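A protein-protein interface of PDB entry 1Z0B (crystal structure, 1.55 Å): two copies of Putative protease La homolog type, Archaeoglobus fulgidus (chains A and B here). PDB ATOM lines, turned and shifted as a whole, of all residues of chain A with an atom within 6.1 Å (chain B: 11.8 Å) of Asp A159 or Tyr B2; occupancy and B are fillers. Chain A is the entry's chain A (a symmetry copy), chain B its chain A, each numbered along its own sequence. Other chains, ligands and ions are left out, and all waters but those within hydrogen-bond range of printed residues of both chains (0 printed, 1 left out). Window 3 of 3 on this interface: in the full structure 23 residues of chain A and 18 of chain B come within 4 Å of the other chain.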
ATOM      1  N   PRO A 131      16.430  18.321 -13.829  1.00  0.00           N
ATOM      2  CA  PRO A 131      15.073  18.769 -13.469  1.00  0.00           C
ATOM      3  C   PRO A 131      14.760  20.191 -13.930  1.00  0.00           C
ATOM      4  O   PRO A 131      15.676  21.018 -14.153  1.00  0.00           O
ATOM      5  CB  PRO A 131      15.048  18.627 -11.926  1.00  0.00           C
ATOM      6  CG  PRO A 131      16.465  18.720 -11.525  1.00  0.00           C
ATOM      7  CD  PRO A 131      17.255  18.074 -12.624  1.00  0.00           C
ATOM      8  N   VAL A 132      13.453  20.441 -14.081  1.00  0.00           N
ATOM      9  CA  VAL A 132      12.867  21.697 -14.542  1.00  0.00           C
ATOM     10  C   VAL A 132      11.683  22.071 -13.664  1.00  0.00           C
ATOM     11  O   VAL A 132      11.204  21.260 -12.866  1.00  0.00           O
ATOM     12  CB  VAL A 132      12.375  21.586 -16.006  1.00  0.00           C
ATOM     13  CG1 VAL A 132      13.547  21.469 -16.959  1.00  0.00           C
ATOM     14  CG2 VAL A 132      11.446  20.399 -16.188  1.00  0.00           C
ATOM     15  N   GLY A 133      11.234  23.304 -13.789  1.00  0.00           N
ATOM     16  CA  GLY A 133      10.054  23.743 -13.055  1.00  0.00           C
ATOM     17  C   GLY A 133       8.750  23.469 -13.782  1.00  0.00           C
ATOM     18  O   GLY A 133       8.694  23.194 -14.989  1.00  0.00           O
ATOM     19  N   GLY A 134       7.667  23.548 -13.032  1.00  0.00           N
ATOM     20  CA  GLY A 134       6.335  23.498 -13.635  1.00  0.00           C
ATOM     21  C   GLY A 134       5.890  22.161 -14.209  1.00  0.00           C
ATOM     22  O   GLY A 134       5.040  22.108 -15.111  1.00  0.00           O
ATOM     23  N   VAL A 135       6.453  21.071 -13.712  1.00  0.00           N
ATOM     24  CA  VAL A 135       6.189  19.763 -14.321  1.00  0.00           C
ATOM     25  C   VAL A 135       4.703  19.373 -14.315  1.00  0.00           C
ATOM     26  O   VAL A 135       4.209  18.836 -15.314  1.00  0.00           O
ATOM     27  CB  VAL A 135       7.127  18.679 -13.763  1.00  0.00           C
ATOM     28  CG1 VAL A 135       6.651  17.309 -14.142  1.00  0.00           C
ATOM     29  CG2 VAL A 135       8.509  18.902 -14.357  1.00  0.00           C
ATOM     30  N   THR A 136       3.993  19.630 -13.211  1.00  0.00           N
ATOM     31  CA  THR A 136       2.554  19.263 -13.101  1.00  0.00           C
ATOM     32  C   THR A 136       1.737  19.999 -14.143  1.00  0.00           C
ATOM     33  O   THR A 136       0.917  19.410 -14.846  1.00  0.00           O
ATOM     34  CB  THR A 136       2.028  19.575 -11.706  1.00  0.00           C
ATOM     35  OG1 THR A 136       2.563  18.604 -10.818  1.00  0.00           O
ATOM     36  CG2 THR A 136       0.525  19.510 -11.649  1.00  0.00           C
ATOM     37  N   ASP A 155      14.130  13.409 -11.450  1.00  0.00           N
ATOM     38  CA  ASP A 155      14.229  14.177 -10.218  1.00  0.00           C
ATOM     39  C   ASP A 155      12.983  15.030 -10.001  1.00  0.00           C
ATOM     40  O   ASP A 155      12.825  15.650  -8.959  1.00  0.00           O
ATOM     41  CB  ASP A 155      15.510  15.032 -10.179  1.00  0.00           C
ATOM     42  CG  ASP A 155      16.775  14.192 -10.042  1.00  0.00           C
ATOM     43  OD1 ASP A 155      16.826  13.367  -9.093  1.00  0.00           O
ATOM     44  OD2 ASP A 155      17.731  14.365 -10.861  1.00  0.00           O
ATOM     45  N   ASN A 156      12.084  15.042 -10.988  1.00  0.00           N
ATOM     46  CA  ASN A 156      10.828  15.775 -10.874  1.00  0.00           C
ATOM     47  C   ASN A 156       9.642  14.865 -10.552  1.00  0.00           C
ATOM     48  O   ASN A 156       8.510  15.344 -10.485  1.00  0.00           O
ATOM     49  CB  ASN A 156      10.523  16.539 -12.171  1.00  0.00           C
ATOM     50  CG  ASN A 156      11.370  17.789 -12.335  1.00  0.00           C
ATOM     51  OD1 ASN A 156      11.988  17.976 -13.369  1.00  0.00           O
ATOM     52  ND2 ASN A 156      11.374  18.659 -11.335  1.00  0.00           N
ATOM     53  N   ILE A 157       9.889  13.575 -10.360  1.00  0.00           N
ATOM     54  CA  ILE A 157       8.810  12.637 -10.131  1.00  0.00           C
ATOM     55  C   ILE A 157       7.962  13.039  -8.919  1.00  0.00           C
ATOM     56  O   ILE A 157       6.746  12.953  -8.954  1.00  0.00           O
ATOM     57  CB  ILE A 157       9.338  11.181 -10.055  1.00  0.00           C
ATOM     58  CG1 ILE A 157       9.166  10.492 -11.414  1.00  0.00           C
ATOM     59  CG2 ILE A 157       8.690  10.381  -8.910  1.00  0.00           C
ATOM     60  CD1 ILE A 157       7.708  10.114 -11.783  1.00  0.00           C
ATOM     61  N   ASP A 158       8.589  13.570  -7.890  1.00  0.00           N
ATOM     62  CA  ASP A 158       7.844  13.903  -6.703  1.00  0.00           C
ATOM     63  C   ASP A 158       7.171  15.269  -6.844  1.00  0.00           C
ATOM     64  O   ASP A 158       6.492  15.739  -5.919  1.00  0.00           O
ATOM     65  CB  ASP A 158       8.781  13.917  -5.513  1.00  0.00           C
ATOM     66  CG  ASP A 158       9.814  14.981  -5.638  1.00  0.00           C
ATOM     67  OD1 ASP A 158      10.423  15.085  -6.733  1.00  0.00           O
ATOM     68  OD2 ASP A 158       9.994  15.737  -4.658  1.00  0.00           O
ATOM     69  N   ASP A 159       7.366  15.919  -7.992  1.00  0.00           N
ATOM     70  CA  ASP A 159       6.693  17.192  -8.283  1.00  0.00           C
ATOM     71  C   ASP A 159       5.331  17.037  -8.964  1.00  0.00           C
ATOM     72  O   ASP A 159       4.628  18.035  -9.184  1.00  0.00           O
ATOM     73  CB  ASP A 159       7.603  18.107  -9.104  1.00  0.00           C
ATOM     74  CG  ASP A 159       8.815  18.518  -8.330  1.00  0.00           C
ATOM     75  OD1 ASP A 159       8.625  19.126  -7.250  1.00  0.00           O
ATOM     76  OD2 ASP A 159       9.946  18.199  -8.765  1.00  0.00           O
ATOM     77  N   VAL A 160       4.951  15.799  -9.276  1.00  0.00           N
ATOM     78  CA  VAL A 160       3.704  15.523  -9.975  1.00  0.00           C
ATOM     79  C   VAL A 160       2.524  15.462  -9.005  1.00  0.00           C
ATOM     80  O   VAL A 160       2.537  14.689  -8.052  1.00  0.00           O
ATOM     81  CB  VAL A 160       3.808  14.223 -10.750  1.00  0.00           C
ATOM     82  CG1 VAL A 160       2.564  13.990 -11.562  1.00  0.00           C
ATOM     83  CG2 VAL A 160       5.027  14.269 -11.672  1.00  0.00           C
ATOM     84  N   LEU A 161       1.512  16.291  -9.233  1.00  0.00           N
ATOM     85  CA  LEU A 161       0.319  16.289  -8.385  1.00  0.00           C
ATOM     86  C   LEU A 161      -0.889  16.581  -9.262  1.00  0.00           C
ATOM     87  O   LEU A 161      -1.203  17.734  -9.519  1.00  0.00           O
ATOM     88  CB  LEU A 161       0.482  17.337  -7.268  1.00  0.00           C
ATOM     89  CG  LEU A 161      -0.608  17.569  -6.215  1.00  0.00           C
ATOM     90  CD1 LEU A 161      -0.818  16.367  -5.354  1.00  0.00           C
ATOM     91  CD2 LEU A 161      -0.169  18.713  -5.324  1.00  0.00           C
ATOM     92  N   TYR B   2      12.155  20.983  -6.658  1.00  0.00           N
ATOM     93  CA  TYR B   2      13.426  20.451  -7.266  1.00  0.00           C
ATOM     94  C   TYR B   2      14.664  21.335  -6.998  1.00  0.00           C
ATOM     95  O   TYR B   2      14.548  22.500  -6.566  1.00  0.00           O
ATOM     96  CB  TYR B   2      13.250  20.247  -8.778  1.00  0.00           C
ATOM     97  CG  TYR B   2      13.424  21.510  -9.600  1.00  0.00           C
ATOM     98  CD1 TYR B   2      12.400  22.448  -9.713  1.00  0.00           C
ATOM     99  CD2 TYR B   2      14.620  21.764 -10.268  1.00  0.00           C
ATOM    100  CE1 TYR B   2      12.571  23.609 -10.472  1.00  0.00           C
ATOM    101  CE2 TYR B   2      14.796  22.905 -11.032  1.00  0.00           C
ATOM    102  CZ  TYR B   2      13.775  23.826 -11.132  1.00  0.00           C
ATOM    103  OH  TYR B   2      13.973  24.968 -11.897  1.00  0.00           O
ATOM    104  N   LYS B   3      15.839  20.768  -7.291  1.00  0.00           N
ATOM    105  CA  LYS B   3      17.147  21.438  -7.139  1.00  0.00           C
ATOM    106  C   LYS B   3      18.032  21.220  -8.354  1.00  0.00           C
ATOM    107  O   LYS B   3      18.035  20.149  -8.966  1.00  0.00           O
ATOM    108  CB  LYS B   3      17.887  20.915  -5.904  1.00  0.00           C
ATOM    109  CG  LYS B   3      17.856  21.906  -4.774  1.00  0.00           C
ATOM    110  CD  LYS B   3      17.529  21.206  -3.461  1.00  0.00           C
ATOM    111  CE  LYS B   3      17.118  22.238  -2.383  1.00  0.00           C
ATOM    112  NZ  LYS B   3      16.020  23.179  -2.850  1.00  0.00           N
ATOM    113  N   LEU B   4      18.816  22.236  -8.679  1.00  0.00           N
ATOM    114  CA  LEU B   4      19.719  22.132  -9.814  1.00  0.00           C
ATOM    115  C   LEU B   4      21.155  21.676  -9.454  1.00  0.00           C
ATOM    116  O   LEU B   4      21.960  21.411 -10.346  1.00  0.00           O
ATOM    117  CB  LEU B   4      19.678  23.421 -10.640  1.00  0.00           C
ATOM    118  CG  LEU B   4      18.322  23.577 -11.357  1.00  0.00           C
ATOM    119  CD1 LEU B   4      18.130  24.992 -11.862  1.00  0.00           C
ATOM    120  CD2 LEU B   4      18.129  22.555 -12.505  1.00  0.00           C
ATOM    121  N   PHE B   5      21.455  21.564  -8.160  1.00  0.00           N
ATOM    122  CA  PHE B   5      22.733  21.017  -7.685  1.00  0.00           C
ATOM    123  C   PHE B   5      22.535  19.658  -7.005  1.00  0.00           C
ATOM    124  O   PHE B   5      21.451  19.341  -6.489  1.00  0.00           O
ATOM    125  CB  PHE B   5      23.416  21.995  -6.710  1.00  0.00           C
ATOM    126  CG  PHE B   5      22.490  22.541  -5.647  1.00  0.00           C
ATOM    127  CD1 PHE B   5      22.238  21.818  -4.489  1.00  0.00           C
ATOM    128  CD2 PHE B   5      21.853  23.771  -5.823  1.00  0.00           C
ATOM    129  CE1 PHE B   5      21.368  22.306  -3.523  1.00  0.00           C
ATOM    130  CE2 PHE B   5      20.979  24.270  -4.857  1.00  0.00           C
ATOM    131  CZ  PHE B   5      20.737  23.535  -3.711  1.00  0.00           C
ATOM    132  N   ILE B   6      23.593  18.860  -7.029  1.00  0.00           N
ATOM    133  CA  ILE B   6      23.668  17.598  -6.306  1.00  0.00           C
ATOM    134  C   ILE B   6      24.507  17.924  -5.079  1.00  0.00           C
ATOM    135  O   ILE B   6      25.472  18.696  -5.193  1.00  0.00           O
ATOM    136  CB  ILE B   6      24.347  16.544  -7.192  1.00  0.00           C
ATOM    137  CG1 ILE B   6      23.495  16.339  -8.454  1.00  0.00           C
ATOM    138  CG2 ILE B   6      24.528  15.258  -6.448  1.00  0.00           C
ATOM    139  CD1 ILE B   6      24.160  15.544  -9.601  1.00  0.00           C
ATOM    140  N   THR B   7      24.149  17.388  -3.910  1.00  0.00           N
ATOM    141  CA  THR B   7      24.842  17.755  -2.681  1.00  0.00           C
ATOM    142  C   THR B   7      25.805  16.703  -2.178  1.00  0.00           C
ATOM    143  O   THR B   7      26.593  16.977  -1.289  1.00  0.00           O
ATOM    144  CB  THR B   7      23.870  18.072  -1.533  1.00  0.00           C
ATOM    145  OG1 THR B   7      23.265  16.853  -1.064  1.00  0.00           O
ATOM    146  CG2 THR B   7      22.786  19.036  -1.980  1.00  0.00           C
ATOM    147  N   ARG B  14      31.294  17.882 -13.350  1.00  0.00           N
ATOM    148  CA  ARG B  14      30.323  18.742 -12.680  1.00  0.00           C
ATOM    149  C   ARG B  14      30.905  19.269 -11.386  1.00  0.00           C
ATOM    150  O   ARG B  14      31.483  18.507 -10.595  1.00  0.00           O
ATOM    151  CB  ARG B  14      29.056  17.959 -12.406  1.00  0.00           C
ATOM    152  CG  ARG B  14      27.961  18.809 -11.858  1.00  0.00           C
ATOM    153  CD  ARG B  14      26.650  18.038 -11.874  1.00  0.00           C
ATOM    154  NE  ARG B  14      25.641  18.883 -11.269  1.00  0.00           N
ATOM    155  CZ  ARG B  14      24.342  18.877 -11.550  1.00  0.00           C
ATOM    156  NH1 ARG B  14      23.828  18.036 -12.436  1.00  0.00           N
ATOM    157  NH2 ARG B  14      23.550  19.730 -10.926  1.00  0.00           N
ATOM    158  N   VAL B  28      24.394  28.945  -5.461  1.00  0.00           N
ATOM    159  CA  VAL B  28      25.142  27.807  -5.980  1.00  0.00           C
ATOM    160  C   VAL B  28      24.916  27.815  -7.473  1.00  0.00           C
ATOM    161  O   VAL B  28      23.773  27.864  -7.935  1.00  0.00           O
ATOM    162  CB  VAL B  28      24.676  26.484  -5.369  1.00  0.00           C
ATOM    163  CG1 VAL B  28      25.447  25.342  -5.956  1.00  0.00           C
ATOM    164  CG2 VAL B  28      24.864  26.517  -3.853  1.00  0.00           C
ATOM    165  N   PRO B  30      26.063  25.482 -10.342  1.00  0.00           N
ATOM    166  CA  PRO B  30      26.790  24.329 -10.859  1.00  0.00           C
ATOM    167  C   PRO B  30      27.244  24.526 -12.302  1.00  0.00           C
ATOM    168  O   PRO B  30      26.543  25.156 -13.118  1.00  0.00           O
ATOM    169  CB  PRO B  30      25.769  23.181 -10.773  1.00  0.00           C
ATOM    170  CG  PRO B  30      24.707  23.677  -9.847  1.00  0.00           C
ATOM    171  CD  PRO B  30      24.649  25.160 -10.062  1.00  0.00           C
ATOM    172  N   GLN B  83      28.527  24.499 -19.532  1.00  0.00           N
ATOM    173  CA  GLN B  83      27.123  24.704 -19.206  1.00  0.00           C
ATOM    174  C   GLN B  83      26.976  25.226 -17.799  1.00  0.00           C
ATOM    175  O   GLN B  83      27.511  24.657 -16.860  1.00  0.00           O
ATOM    176  CB  GLN B  83      26.391  23.378 -19.312  1.00  0.00           C
ATOM    177  CG  GLN B  83      24.965  23.364 -18.702  1.00  0.00           C
ATOM    178  CD  GLN B  83      24.251  22.099 -18.998  1.00  0.00           C
ATOM    179  OE1 GLN B  83      24.861  21.062 -19.197  1.00  0.00           O
ATOM    180  NE2 GLN B  83      22.922  22.163 -19.041  1.00  0.00           N
ATOM    181  N   PHE B  84      26.231  26.316 -17.655  1.00  0.00           N
ATOM    182  CA  PHE B  84      25.867  26.845 -16.358  1.00  0.00           C
ATOM    183  C   PHE B  84      24.473  26.332 -16.035  1.00  0.00           C
ATOM    184  O   PHE B  84      23.541  26.527 -16.825  1.00  0.00           O
ATOM    185  CB  PHE B  84      25.880  28.360 -16.407  1.00  0.00           C
ATOM    186  CG  PHE B  84      27.250  28.944 -16.687  1.00  0.00           C
ATOM    187  CD1 PHE B  84      28.159  29.151 -15.653  1.00  0.00           C
ATOM    188  CD2 PHE B  84      27.641  29.272 -17.981  1.00  0.00           C
ATOM    189  CE1 PHE B  84      29.453  29.688 -15.899  1.00  0.00           C
ATOM    190  CE2 PHE B  84      28.924  29.831 -18.250  1.00  0.00           C
ATOM    191  CZ  PHE B  84      29.824  30.037 -17.203  1.00  0.00           C
ATOM    192  N   VAL B  85      24.335  25.642 -14.916  1.00  0.00           N
ATOM    193  CA  VAL B  85      23.040  25.089 -14.507  1.00  0.00           C
ATOM    194  C   VAL B  85      22.216  26.107 -13.699  1.00  0.00           C
ATOM    195  O   VAL B  85      22.602  26.523 -12.600  1.00  0.00           O
ATOM    196  CB  VAL B  85      23.224  23.806 -13.713  1.00  0.00           C
ATOM    197  CG1 VAL B  85      21.889  23.230 -13.357  1.00  0.00           C
ATOM    198  CG2 VAL B  85      24.015  22.802 -14.518  1.00  0.00           C
ATOM    199  N   GLY B  86      21.066  26.468 -14.249  1.00  0.00           N
ATOM    200  CA  GLY B  86      20.224  27.519 -13.698  1.00  0.00           C
ATOM    201  C   GLY B  86      20.555  28.849 -14.354  1.00  0.00           C
ATOM    202  O   GLY B  86      21.630  29.433 -14.104  1.00  0.00           O
ATOM    203  N   THR B  87      19.651  29.330 -15.208  1.00  0.00           N
ATOM    204  CA  THR B  87      19.774  30.698 -15.747  1.00  0.00           C
ATOM    205  C   THR B  87      19.227  31.770 -14.781  1.00  0.00           C
ATOM    206  O   THR B  87      18.087  31.680 -14.296  1.00  0.00           O
ATOM    207  CB  THR B  87      19.122  30.850 -17.159  1.00  0.00           C
ATOM    208  OG1 THR B  87      19.347  32.185 -17.638  1.00  0.00           O
ATOM    209  CG2 THR B  87      17.599  30.559 -17.134  1.00  0.00           C
ATOM    210  N   TYR B  88      20.048  32.771 -14.485  1.00  0.00           N
ATOM    211  CA  TYR B  88      19.595  33.866 -13.647  1.00  0.00           C
ATOM    212  C   TYR B  88      19.988  35.168 -14.286  1.00  0.00           C
ATOM    213  O   TYR B  88      21.071  35.305 -14.883  1.00  0.00           O
ATOM    214  CB  TYR B  88      20.206  33.836 -12.248  1.00  0.00           C
ATOM    215  CG  TYR B  88      20.147  32.524 -11.514  1.00  0.00           C
ATOM    216  CD1 TYR B  88      21.244  31.648 -11.536  1.00  0.00           C
ATOM    217  CD2 TYR B  88      19.012  32.161 -10.768  1.00  0.00           C
ATOM    218  CE1 TYR B  88      21.210  30.432 -10.852  1.00  0.00           C
ATOM    219  CE2 TYR B  88      18.967  30.945 -10.074  1.00  0.00           C
ATOM    220  CZ  TYR B  88      20.076  30.089 -10.126  1.00  0.00           C
ATOM    221  OH  TYR B  88      20.053  28.888  -9.456  1.00  0.00           O
ATOM    222  N   GLN B 144      23.140  27.005   2.838  1.00  0.00           N
ATOM    223  CA  GLN B 144      21.717  26.830   2.568  1.00  0.00           C
ATOM    224  C   GLN B 144      21.389  25.684   1.619  1.00  0.00           C
ATOM    225  O   GLN B 144      20.302  25.109   1.704  1.00  0.00           O
ATOM    226  CB  GLN B 144      21.162  28.119   2.030  1.00  0.00           C
ATOM    227  CG  GLN B 144      21.268  29.230   3.037  1.00  0.00           C
ATOM    228  CD  GLN B 144      21.111  30.565   2.423  1.00  0.00           C
ATOM    229  OE1 GLN B 144      20.979  30.695   1.197  1.00  0.00           O
ATOM    230  NE2 GLN B 144      21.112  31.595   3.259  1.00  0.00           N
ATOM    231  N   ALA B 145      22.322  25.355   0.722  1.00  0.00           N
ATOM    232  CA  ALA B 145      22.195  24.209  -0.179  1.00  0.00           C
ATOM    233  C   ALA B 145      22.550  22.863   0.496  1.00  0.00           C
ATOM    234  O   ALA B 145      22.401  21.803  -0.117  1.00  0.00           O
ATOM    235  CB  ALA B 145      23.075  24.428  -1.410  1.00  0.00           C
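Pro A131 touches just these residues of chain B: Tyr B2 (3.6 Å), Lys B3 (3.3 Å) and Leu B4 (3.3 Å). Gly A134 touches none of the printed residues of chain B. No residue of chain B comes within 4 Å of Ile A157. No residue of chain B comes within 4 Å of Asp A158. Asp A159 touches just one residue of chain B: Tyr B2. No residue of chain B comes within 4 Å of Val A160. Of chain A, only Pro A131 (3.6 Å), Val A132 (3.6 Å), Gly A133 (3.6 Å), Asn A156 (3.5 Å) and Asp A159 (3.9 Å) come within 4 Å of Tyr B2. Of the printed residues of chain A, Lys B3 touches Pro A131. Printed residues of chain A within 4 Å of Leu B4: Pro A131. Thr B7 touches none of the printed residues of chain A. Thr B87 touches none of the printed residues of chain A. The nearest residue of chain B that does not touch Asp A159 is Lys B3 (6.6 Å). The nearest residue of chain A that does not touch Tyr B2 is Asp A155 (4.6 Å).
N of Val A132 sits at hydrogen-bond distance from OD1 of Asn A156, 3.0 Å away. The side-chain amide nitrogen of Asn A156 lies within hydrogen-bond range of the side-chain carboxylate of Asp A159. OG1 of Thr A136 sits at hydrogen-bond distance from O of Asp A159, at 2.7 Å.
Hydrophobic or aromatic side chains of chain B that line the printed part of chain A: Tyr B2 and Leu B4. Printed residues of chain A that touch a printed residue of chain B: Pro A131, Val A132, Gly A133, Asn A156 and Asp A159. Hydrophobic or aromatic side chains of chain A that line the printed part of chain B: Pro A131. Among the printed residues, 7 pairs touch across the chains.
No position is printed for both chains. Of the 7 pairs that touch across the chains among the printed residues, none has its exchanged pair printed and touching as well.
Among the printed residues, pairs that only touch across the chains: Pro A131 with Lys B3 (3.3 Å), Pro A131 with Leu B4 (3.3 Å), Asn A156 with Tyr B2 (3.5 Å), Pro A131 with Tyr B2 (3.6 Å), Val A132 with Tyr B2 (3.6 Å), Gly A133 with Tyr B2 (3.6 Å) and Asp A159 with Tyr B2 (3.9 Å).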
